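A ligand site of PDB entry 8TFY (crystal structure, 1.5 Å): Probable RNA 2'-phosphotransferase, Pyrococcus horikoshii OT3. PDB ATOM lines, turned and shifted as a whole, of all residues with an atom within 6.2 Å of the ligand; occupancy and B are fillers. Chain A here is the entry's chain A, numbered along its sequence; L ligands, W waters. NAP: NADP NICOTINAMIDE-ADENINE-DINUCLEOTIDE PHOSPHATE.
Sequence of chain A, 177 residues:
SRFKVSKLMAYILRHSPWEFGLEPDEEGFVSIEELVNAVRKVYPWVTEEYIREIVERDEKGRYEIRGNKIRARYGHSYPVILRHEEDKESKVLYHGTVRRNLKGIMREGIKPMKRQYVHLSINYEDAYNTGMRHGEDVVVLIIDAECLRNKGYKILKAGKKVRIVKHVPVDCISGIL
O of Ser 6 lies within hydrogen-bond range of OH of Tyr 63, 2.8 Å away.
The guanidinium group of Arg 14 sits at hydrogen-bond distance from the backbone carbonyl oxygen of Tyr 74 (3.1 Å).
The backbone NH (N) of Lys 60 is in hydrogen-bond range of the side-chain carboxylate (OD1) of Asp 58, 2.9 Å away.
The side-chain carboxylate of Asp 58 lies within salt-bridge range of the guanidinium group of Arg 62 (2.8 Å).
Phe 3 touches the ligand (CD1 to N6A, 3.6 Å).
Ala 10 touches the ligand.
OH of Tyr 63 touches C2A of the ligand, at 3.5 Å.
Hydrophobic or aromatic side chains within 4 Å of the ligand: Phe 3, Ala 10 and Tyr 74.
Ten residues have an atom within 4 Å of the ligand: Phe 3, Ser 6, Lys 7, Ala 10, Arg 14, Lys 60, Arg 62, Tyr 63, Tyr 74 and Arg 133.
Along chain A the residues within 4 Å of the ligand span positions 3 to 133.
A nitrogen (N1A) of the ligand sits at hydrogen-bond distance from the side-chain hydroxyl of Ser 6, 2.6 Å away.
NZ of Lys 7 is in salt-bridge range of O5D of the ligand, 2.7 Å away.
An oxygen (O1X) of the ligand sits at hydrogen-bond distance from the side-chain hydroxyl (OH) of Tyr 74, 2.7 Å away.
The side-chain amino group (NZ) of Lys 60 is in salt-bridge range of an oxygen (O2X) of the ligand.
O1X of the ligand lies within salt-bridge range of NE of Arg 62, 2.8 Å away.
The guanidinium group (NH2) of Arg 14 lies within salt-bridge range of an oxygen (O1X) of the ligand (2.8 Å).
The guanidinium group (NH1) of Arg 133 is in salt-bridge range of an oxygen (O3X) of the ligand (2.9 Å).
Water W2 bridges an oxygen (O2A) of the ligand (2.6 Å) and the side-chain amino group of Lys 60 (3.4 Å).
Water W6 bridges an oxygen (O3B) of the ligand (2.8 Å) and the guanidinium group of Arg 133 (3.3 Å).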
ATOM      1  N   ARG A   2      14.745  -0.657 -29.045  1.00  0.00           N
ATOM      2  CA  ARG A   2      14.552  -1.183 -27.687  1.00  0.00           C
ATOM      3  C   ARG A   2      13.157  -0.864 -27.155  1.00  0.00           C
ATOM      4  O   ARG A   2      12.540  -1.699 -26.487  1.00  0.00           O
ATOM      5  CB  ARG A   2      15.593  -0.619 -26.720  1.00  0.00           C
ATOM      6  CG  ARG A   2      16.710  -1.553 -26.332  1.00  0.00           C
ATOM      7  CD  ARG A   2      17.808  -0.794 -25.580  1.00  0.00           C
ATOM      8  NE  ARG A   2      17.282  -0.284 -24.310  1.00  0.00           N
ATOM      9  CZ  ARG A   2      17.423   0.976 -23.919  1.00  0.00           C
ATOM     10  NH1 ARG A   2      18.134   1.846 -24.624  1.00  0.00           N
ATOM     11  NH2 ARG A   2      16.844   1.373 -22.784  1.00  0.00           N
ATOM     12  N   PHE A   3      12.657   0.335 -27.425  1.00  0.00           N
ATOM     13  CA  PHE A   3      11.340   0.698 -26.902  1.00  0.00           C
ATOM     14  C   PHE A   3      10.232  -0.179 -27.480  1.00  0.00           C
ATOM     15  O   PHE A   3       9.395  -0.699 -26.736  1.00  0.00           O
ATOM     16  CB  PHE A   3      11.076   2.176 -27.201  1.00  0.00           C
ATOM     17  CG  PHE A   3       9.685   2.604 -26.866  1.00  0.00           C
ATOM     18  CD1 PHE A   3       9.322   2.850 -25.544  1.00  0.00           C
ATOM     19  CD2 PHE A   3       8.732   2.765 -27.860  1.00  0.00           C
ATOM     20  CE1 PHE A   3       8.034   3.267 -25.223  1.00  0.00           C
ATOM     21  CE2 PHE A   3       7.432   3.164 -27.544  1.00  0.00           C
ATOM     22  CZ  PHE A   3       7.085   3.402 -26.233  1.00  0.00           C
ATOM     23  N   SER A   6      10.591  -3.766 -26.170  1.00  0.00           N
ATOM     24  CA  SER A   6      10.282  -3.821 -24.742  1.00  0.00           C
ATOM     25  C   SER A   6       8.790  -3.704 -24.501  1.00  0.00           C
ATOM     26  O   SER A   6       8.241  -4.379 -23.633  1.00  0.00           O
ATOM     27  CB  SER A   6      11.043  -2.739 -23.976  1.00  0.00           C
ATOM     28  OG  SER A   6      10.785  -2.802 -22.582  1.00  0.00           O
ATOM     29  N   LYS A   7       8.118  -2.823 -25.241  1.00  0.00           N
ATOM     30  CA  LYS A   7       6.672  -2.686 -25.076  1.00  0.00           C
ATOM     31  C   LYS A   7       5.967  -3.993 -25.391  1.00  0.00           C
ATOM     32  O   LYS A   7       5.044  -4.420 -24.664  1.00  0.00           O
ATOM     33  CB  LYS A   7       6.149  -1.555 -25.955  1.00  0.00           C
ATOM     34  CG  LYS A   7       6.500  -0.183 -25.443  1.00  0.00           C
ATOM     35  CD  LYS A   7       5.456   0.313 -24.465  1.00  0.00           C
ATOM     36  CE  LYS A   7       4.173   0.703 -25.186  1.00  0.00           C
ATOM     37  NZ  LYS A   7       3.135   1.201 -24.237  1.00  0.00           N
ATOM     38  N   LEU A   8       6.418  -4.675 -26.449  1.00  0.00           N
ATOM     39  CA  LEU A   8       5.842  -5.987 -26.761  1.00  0.00           C
ATOM     40  C   LEU A   8       6.162  -7.004 -25.671  1.00  0.00           C
ATOM     41  O   LEU A   8       5.300  -7.822 -25.293  1.00  0.00           O
ATOM     42  CB  LEU A   8       6.352  -6.491 -28.113  1.00  0.00           C
ATOM     43  CG  LEU A   8       5.800  -7.862 -28.558  1.00  0.00           C
ATOM     44  CD1 LEU A   8       4.254  -7.862 -28.579  1.00  0.00           C
ATOM     45  CD2 LEU A   8       6.383  -8.288 -29.911  1.00  0.00           C
ATOM     46  N   ALA A  10       6.617  -6.473 -22.547  1.00  0.00           N
ATOM     47  CA  ALA A  10       5.777  -6.192 -21.376  1.00  0.00           C
ATOM     48  C   ALA A  10       4.331  -6.647 -21.612  1.00  0.00           C
ATOM     49  O   ALA A  10       3.692  -7.199 -20.710  1.00  0.00           O
ATOM     50  CB  ALA A  10       5.817  -4.699 -21.038  1.00  0.00           C
ATOM     51  N   TYR A  11       3.826  -6.468 -22.833  1.00  0.00           N
ATOM     52  CA  TYR A  11       2.487  -6.964 -23.150  1.00  0.00           C
ATOM     53  C   TYR A  11       2.407  -8.483 -23.021  1.00  0.00           C
ATOM     54  O   TYR A  11       1.465  -9.019 -22.400  1.00  0.00           O
ATOM     55  CB  TYR A  11       2.113  -6.519 -24.562  1.00  0.00           C
ATOM     56  CG  TYR A  11       0.806  -7.083 -25.070  1.00  0.00           C
ATOM     57  CD1 TYR A  11      -0.412  -6.568 -24.636  1.00  0.00           C
ATOM     58  CD2 TYR A  11       0.801  -8.145 -25.976  1.00  0.00           C
ATOM     59  CE1 TYR A  11      -1.597  -7.087 -25.128  1.00  0.00           C
ATOM     60  CE2 TYR A  11      -0.376  -8.673 -26.450  1.00  0.00           C
ATOM     61  CZ  TYR A  11      -1.576  -8.136 -26.024  1.00  0.00           C
ATOM     62  OH  TYR A  11      -2.762  -8.653 -26.498  1.00  0.00           O
ATOM     63  N   ARG A  14       3.129  -9.501 -19.099  1.00  0.00           N
ATOM     64  CA  ARG A  14       2.160  -9.033 -18.105  1.00  0.00           C
ATOM     65  C   ARG A  14       0.721  -9.391 -18.431  1.00  0.00           C
ATOM     66  O   ARG A  14      -0.087  -9.549 -17.507  1.00  0.00           O
ATOM     67  CB  ARG A  14       2.216  -7.502 -17.956  1.00  0.00           C
ATOM     68  CG  ARG A  14       3.478  -6.926 -17.335  1.00  0.00           C
ATOM     69  CD  ARG A  14       3.499  -5.445 -17.542  1.00  0.00           C
ATOM     70  NE  ARG A  14       4.664  -4.794 -16.941  1.00  0.00           N
ATOM     71  CZ  ARG A  14       4.984  -3.529 -17.157  1.00  0.00           C
ATOM     72  NH1 ARG A  14       4.211  -2.738 -17.891  1.00  0.00           N
ATOM     73  NH2 ARG A  14       6.110  -3.045 -16.633  1.00  0.00           N
ATOM     74  N   HIS A  15       0.376  -9.502 -19.720  1.00  0.00           N
ATOM     75  CA  HIS A  15      -1.038  -9.470 -20.078  1.00  0.00           C
ATOM     76  C   HIS A  15      -1.504 -10.610 -20.962  1.00  0.00           C
ATOM     77  O   HIS A  15      -2.609 -11.099 -20.777  1.00  0.00           O
ATOM     78  CB  HIS A  15      -1.372  -8.137 -20.758  1.00  0.00           C
ATOM     79  CG  HIS A  15      -1.070  -6.958 -19.893  1.00  0.00           C
ATOM     80  ND1 HIS A  15      -1.571  -6.837 -18.613  1.00  0.00           N
ATOM     81  CD2 HIS A  15      -0.325  -5.852 -20.120  1.00  0.00           C
ATOM     82  CE1 HIS A  15      -1.132  -5.704 -18.083  1.00  0.00           C
ATOM     83  NE2 HIS A  15      -0.381  -5.087 -18.977  1.00  0.00           N
ATOM     84  N   ASP A  58      17.134  -1.943 -18.768  1.00  0.00           N
ATOM     85  CA  ASP A  58      15.850  -1.324 -18.479  1.00  0.00           C
ATOM     86  C   ASP A  58      15.938  -0.382 -17.281  1.00  0.00           C
ATOM     87  O   ASP A  58      16.390  -0.774 -16.202  1.00  0.00           O
ATOM     88  CB  ASP A  58      14.778  -2.400 -18.236  1.00  0.00           C
ATOM     89  CG  ASP A  58      13.410  -1.793 -18.022  1.00  0.00           C
ATOM     90  OD1 ASP A  58      13.119  -1.452 -16.848  1.00  0.00           O
ATOM     91  OD2 ASP A  58      12.629  -1.675 -19.004  1.00  0.00           O
ATOM     92  N   GLU A  59      15.455   0.848 -17.472  1.00  0.00           N
ATOM     93  CA  GLU A  59      15.630   1.919 -16.493  1.00  0.00           C
ATOM     94  C   GLU A  59      14.761   1.738 -15.249  1.00  0.00           C
ATOM     95  O   GLU A  59      15.061   2.332 -14.211  1.00  0.00           O
ATOM     96  CB  GLU A  59      15.301   3.269 -17.140  1.00  0.00           C
ATOM     97  CG  GLU A  59      16.292   3.764 -18.169  1.00  0.00           C
ATOM     98  CD  GLU A  59      16.075   3.152 -19.564  1.00  0.00           C
ATOM     99  OE1 GLU A  59      15.119   2.353 -19.729  1.00  0.00           O
ATOM    100  OE2 GLU A  59      16.845   3.507 -20.484  1.00  0.00           O
ATOM    101  N   LYS A  60      13.687   0.962 -15.337  1.00  0.00           N
ATOM    102  CA  LYS A  60      12.818   0.734 -14.193  1.00  0.00           C
ATOM    103  C   LYS A  60      13.026  -0.621 -13.530  1.00  0.00           C
ATOM    104  O   LYS A  60      12.415  -0.891 -12.494  1.00  0.00           O
ATOM    105  CB  LYS A  60      11.347   0.860 -14.602  1.00  0.00           C
ATOM    106  CG  LYS A  60      10.985   2.235 -15.107  1.00  0.00           C
ATOM    107  CD  LYS A  60       9.475   2.373 -15.296  1.00  0.00           C
ATOM    108  CE  LYS A  60       9.119   3.760 -15.820  1.00  0.00           C
ATOM    109  NZ  LYS A  60       7.636   3.955 -15.858  1.00  0.00           N
ATOM    110  N   ARG A  62      12.105  -3.428 -15.108  1.00  0.00           N
ATOM    111  CA  ARG A  62      10.841  -4.085 -15.454  1.00  0.00           C
ATOM    112  C   ARG A  62      10.918  -5.601 -15.457  1.00  0.00           C
ATOM    113  O   ARG A  62       9.890  -6.267 -15.213  1.00  0.00           O
ATOM    114  CB  ARG A  62      10.357  -3.624 -16.830  1.00  0.00           C
ATOM    115  CG  ARG A  62       9.906  -2.189 -16.884  1.00  0.00           C
ATOM    116  CD  ARG A  62       9.306  -1.855 -18.231  1.00  0.00           C
ATOM    117  NE  ARG A  62       8.821  -0.480 -18.257  1.00  0.00           N
ATOM    118  CZ  ARG A  62       9.527   0.562 -18.688  1.00  0.00           C
ATOM    119  NH1 ARG A  62      10.773   0.423 -19.141  1.00  0.00           N
ATOM    120  NH2 ARG A  62       8.968   1.770 -18.693  1.00  0.00           N
ATOM    121  N   TYR A  63      12.087  -6.168 -15.759  1.00  0.00           N
ATOM    122  CA  TYR A  63      12.179  -7.594 -16.043  1.00  0.00           C
ATOM    123  C   TYR A  63      13.171  -8.278 -15.119  1.00  0.00           C
ATOM    124  O   TYR A  63      14.060  -7.652 -14.543  1.00  0.00           O
ATOM    125  CB  TYR A  63      12.625  -7.816 -17.505  1.00  0.00           C
ATOM    126  CG  TYR A  63      11.796  -7.025 -18.489  1.00  0.00           C
ATOM    127  CD1 TYR A  63      10.462  -7.373 -18.745  1.00  0.00           C
ATOM    128  CD2 TYR A  63      12.326  -5.912 -19.145  1.00  0.00           C
ATOM    129  CE1 TYR A  63       9.693  -6.648 -19.617  1.00  0.00           C
ATOM    130  CE2 TYR A  63      11.546  -5.162 -20.031  1.00  0.00           C
ATOM    131  CZ  TYR A  63      10.241  -5.558 -20.270  1.00  0.00           C
ATOM    132  OH  TYR A  63       9.438  -4.842 -21.131  1.00  0.00           O
ATOM    133  N   TYR A  74       6.492  -6.770 -12.275  1.00  0.00           N
ATOM    134  CA  TYR A  74       5.272  -6.156 -11.758  1.00  0.00           C
ATOM    135  C   TYR A  74       4.339  -5.889 -12.925  1.00  0.00           C
ATOM    136  O   TYR A  74       4.698  -6.066 -14.091  1.00  0.00           O
ATOM    137  CB  TYR A  74       5.586  -4.868 -10.984  1.00  0.00           C
ATOM    138  CG  TYR A  74       6.249  -3.778 -11.826  1.00  0.00           C
ATOM    139  CD1 TYR A  74       5.488  -2.921 -12.624  1.00  0.00           C
ATOM    140  CD2 TYR A  74       7.656  -3.621 -11.846  1.00  0.00           C
ATOM    141  CE1 TYR A  74       6.082  -1.937 -13.423  1.00  0.00           C
ATOM    142  CE2 TYR A  74       8.247  -2.621 -12.641  1.00  0.00           C
ATOM    143  CZ  TYR A  74       7.459  -1.774 -13.415  1.00  0.00           C
ATOM    144  OH  TYR A  74       8.046  -0.794 -14.202  1.00  0.00           O
ATOM    145  N   ASN A 129       3.584  10.571 -12.072  1.00  0.00           N
ATOM    146  CA  ASN A 129       3.446  10.142 -13.454  1.00  0.00           C
ATOM    147  C   ASN A 129       2.557   8.909 -13.576  1.00  0.00           C
ATOM    148  O   ASN A 129       1.792   8.778 -14.539  1.00  0.00           O
ATOM    149  CB  ASN A 129       4.818   9.887 -14.061  1.00  0.00           C
ATOM    150  CG  ASN A 129       5.607  11.171 -14.230  1.00  0.00           C
ATOM    151  OD1 ASN A 129       5.024  12.251 -14.316  1.00  0.00           O
ATOM    152  ND2 ASN A 129       6.926  11.061 -14.296  1.00  0.00           N
ATOM    153  N   THR A 130       2.622   8.012 -12.594  1.00  0.00           N
ATOM    154  CA  THR A 130       1.742   6.858 -12.567  1.00  0.00           C
ATOM    155  C   THR A 130       0.294   7.286 -12.390  1.00  0.00           C
ATOM    156  O   THR A 130      -0.606   6.776 -13.075  1.00  0.00           O
ATOM    157  CB  THR A 130       2.164   5.919 -11.437  1.00  0.00           C
ATOM    158  OG1 THR A 130       3.444   5.374 -11.762  1.00  0.00           O
ATOM    159  CG2 THR A 130       1.188   4.781 -11.297  1.00  0.00           C
ATOM    160  N   ARG A 133      -1.879   8.327 -15.330  1.00  0.00           N
ATOM    161  CA  ARG A 133      -2.479   7.318 -16.194  1.00  0.00           C
ATOM    162  C   ARG A 133      -3.983   7.186 -15.974  1.00  0.00           C
ATOM    163  O   ARG A 133      -4.682   6.628 -16.826  1.00  0.00           O
ATOM    164  CB  ARG A 133      -1.799   5.969 -15.959  1.00  0.00           C
ATOM    165  CG  ARG A 133      -0.341   5.986 -16.376  1.00  0.00           C
ATOM    166  CD  ARG A 133       0.343   4.705 -16.049  1.00  0.00           C
ATOM    167  NE  ARG A 133       1.758   4.770 -16.391  1.00  0.00           N
ATOM    168  CZ  ARG A 133       2.640   3.829 -16.076  1.00  0.00           C
ATOM    169  NH1 ARG A 133       2.279   2.731 -15.448  1.00  0.00           N
ATOM    170  NH2 ARG A 133       3.916   4.002 -16.407  1.00  0.00           N
HETATM  171  PA  NAP L   1       2.834   5.081 -20.272  1.00  0.00           P
HETATM  172  O1A NAP L   1       1.596   5.629 -19.644  1.00  0.00           O
HETATM  173  O2A NAP L   1       4.162   5.602 -19.819  1.00  0.00           O
HETATM  174  O5B NAP L   1       2.843   3.495 -20.084  1.00  0.00           O
HETATM  175  C5B NAP L   1       1.708   2.700 -20.473  1.00  0.00           C
HETATM  176  C4B NAP L   1       2.075   1.251 -20.251  1.00  0.00           C
HETATM  177  O4B NAP L   1       3.216   0.964 -21.114  1.00  0.00           O
HETATM  178  C3B NAP L   1       2.522   0.885 -18.821  1.00  0.00           C
HETATM  179  O3B NAP L   1       2.096  -0.435 -18.498  1.00  0.00           O
HETATM  180  C2B NAP L   1       4.041   0.968 -18.931  1.00  0.00           C
HETATM  181  O2B NAP L   1       4.732   0.141 -18.010  1.00  0.00           O
HETATM  182  C1B NAP L   1       4.262   0.434 -20.343  1.00  0.00           C
HETATM  183  N9A NAP L   1       5.542   0.860 -20.891  1.00  0.00           N
HETATM  184  C8A NAP L   1       5.952   2.148 -21.142  1.00  0.00           C
HETATM  185  N7A NAP L   1       7.172   2.222 -21.621  1.00  0.00           N
HETATM  186  C5A NAP L   1       7.597   0.910 -21.667  1.00  0.00           C
HETATM  187  C6A NAP L   1       8.807   0.309 -22.075  1.00  0.00           C
HETATM  188  N6A NAP L   1       9.860   1.000 -22.525  1.00  0.00           N
HETATM  189  N1A NAP L   1       8.894  -1.037 -22.007  1.00  0.00           N
HETATM  190  C2A NAP L   1       7.848  -1.729 -21.546  1.00  0.00           C
HETATM  191  N3A NAP L   1       6.669  -1.286 -21.139  1.00  0.00           N
HETATM  192  C4A NAP L   1       6.605   0.057 -21.230  1.00  0.00           C
HETATM  193  O3  NAP L   1       2.724   5.255 -21.857  1.00  0.00           O
HETATM  194  PN  NAP L   1       3.734   5.220 -23.113  1.00  0.00           P
HETATM  195  O1N NAP L   1       5.047   5.796 -22.700  1.00  0.00           O
HETATM  196  O2N NAP L   1       3.038   5.852 -24.271  1.00  0.00           O
HETATM  197  O5D NAP L   1       3.906   3.650 -23.393  1.00  0.00           O
HETATM  198  P2B NAP L   1       5.636   0.801 -16.834  1.00  0.00           P
HETATM  199  O1X NAP L   1       6.642  -0.293 -16.502  1.00  0.00           O
HETATM  200  O2X NAP L   1       6.313   2.033 -17.394  1.00  0.00           O
HETATM  201  O3X NAP L   1       4.728   1.108 -15.667  1.00  0.00           O
HETATM  202  O   HOH W   1      -0.331  -1.474 -19.825  1.00  0.00           O
HETATM  203  O   HOH W   2       6.354   4.515 -18.997  1.00  0.00           O
HETATM  204  O   HOH W   3      -0.883   6.442 -20.009  1.00  0.00           O
HETATM  205  O   HOH W   4      12.525   0.482 -23.154  1.00  0.00           O
HETATM  206  O   HOH W   5      10.524   3.919 -22.256  1.00  0.00           O
HETATM  207  O   HOH W   6       2.402  -0.599 -15.698  1.00  0.00           O
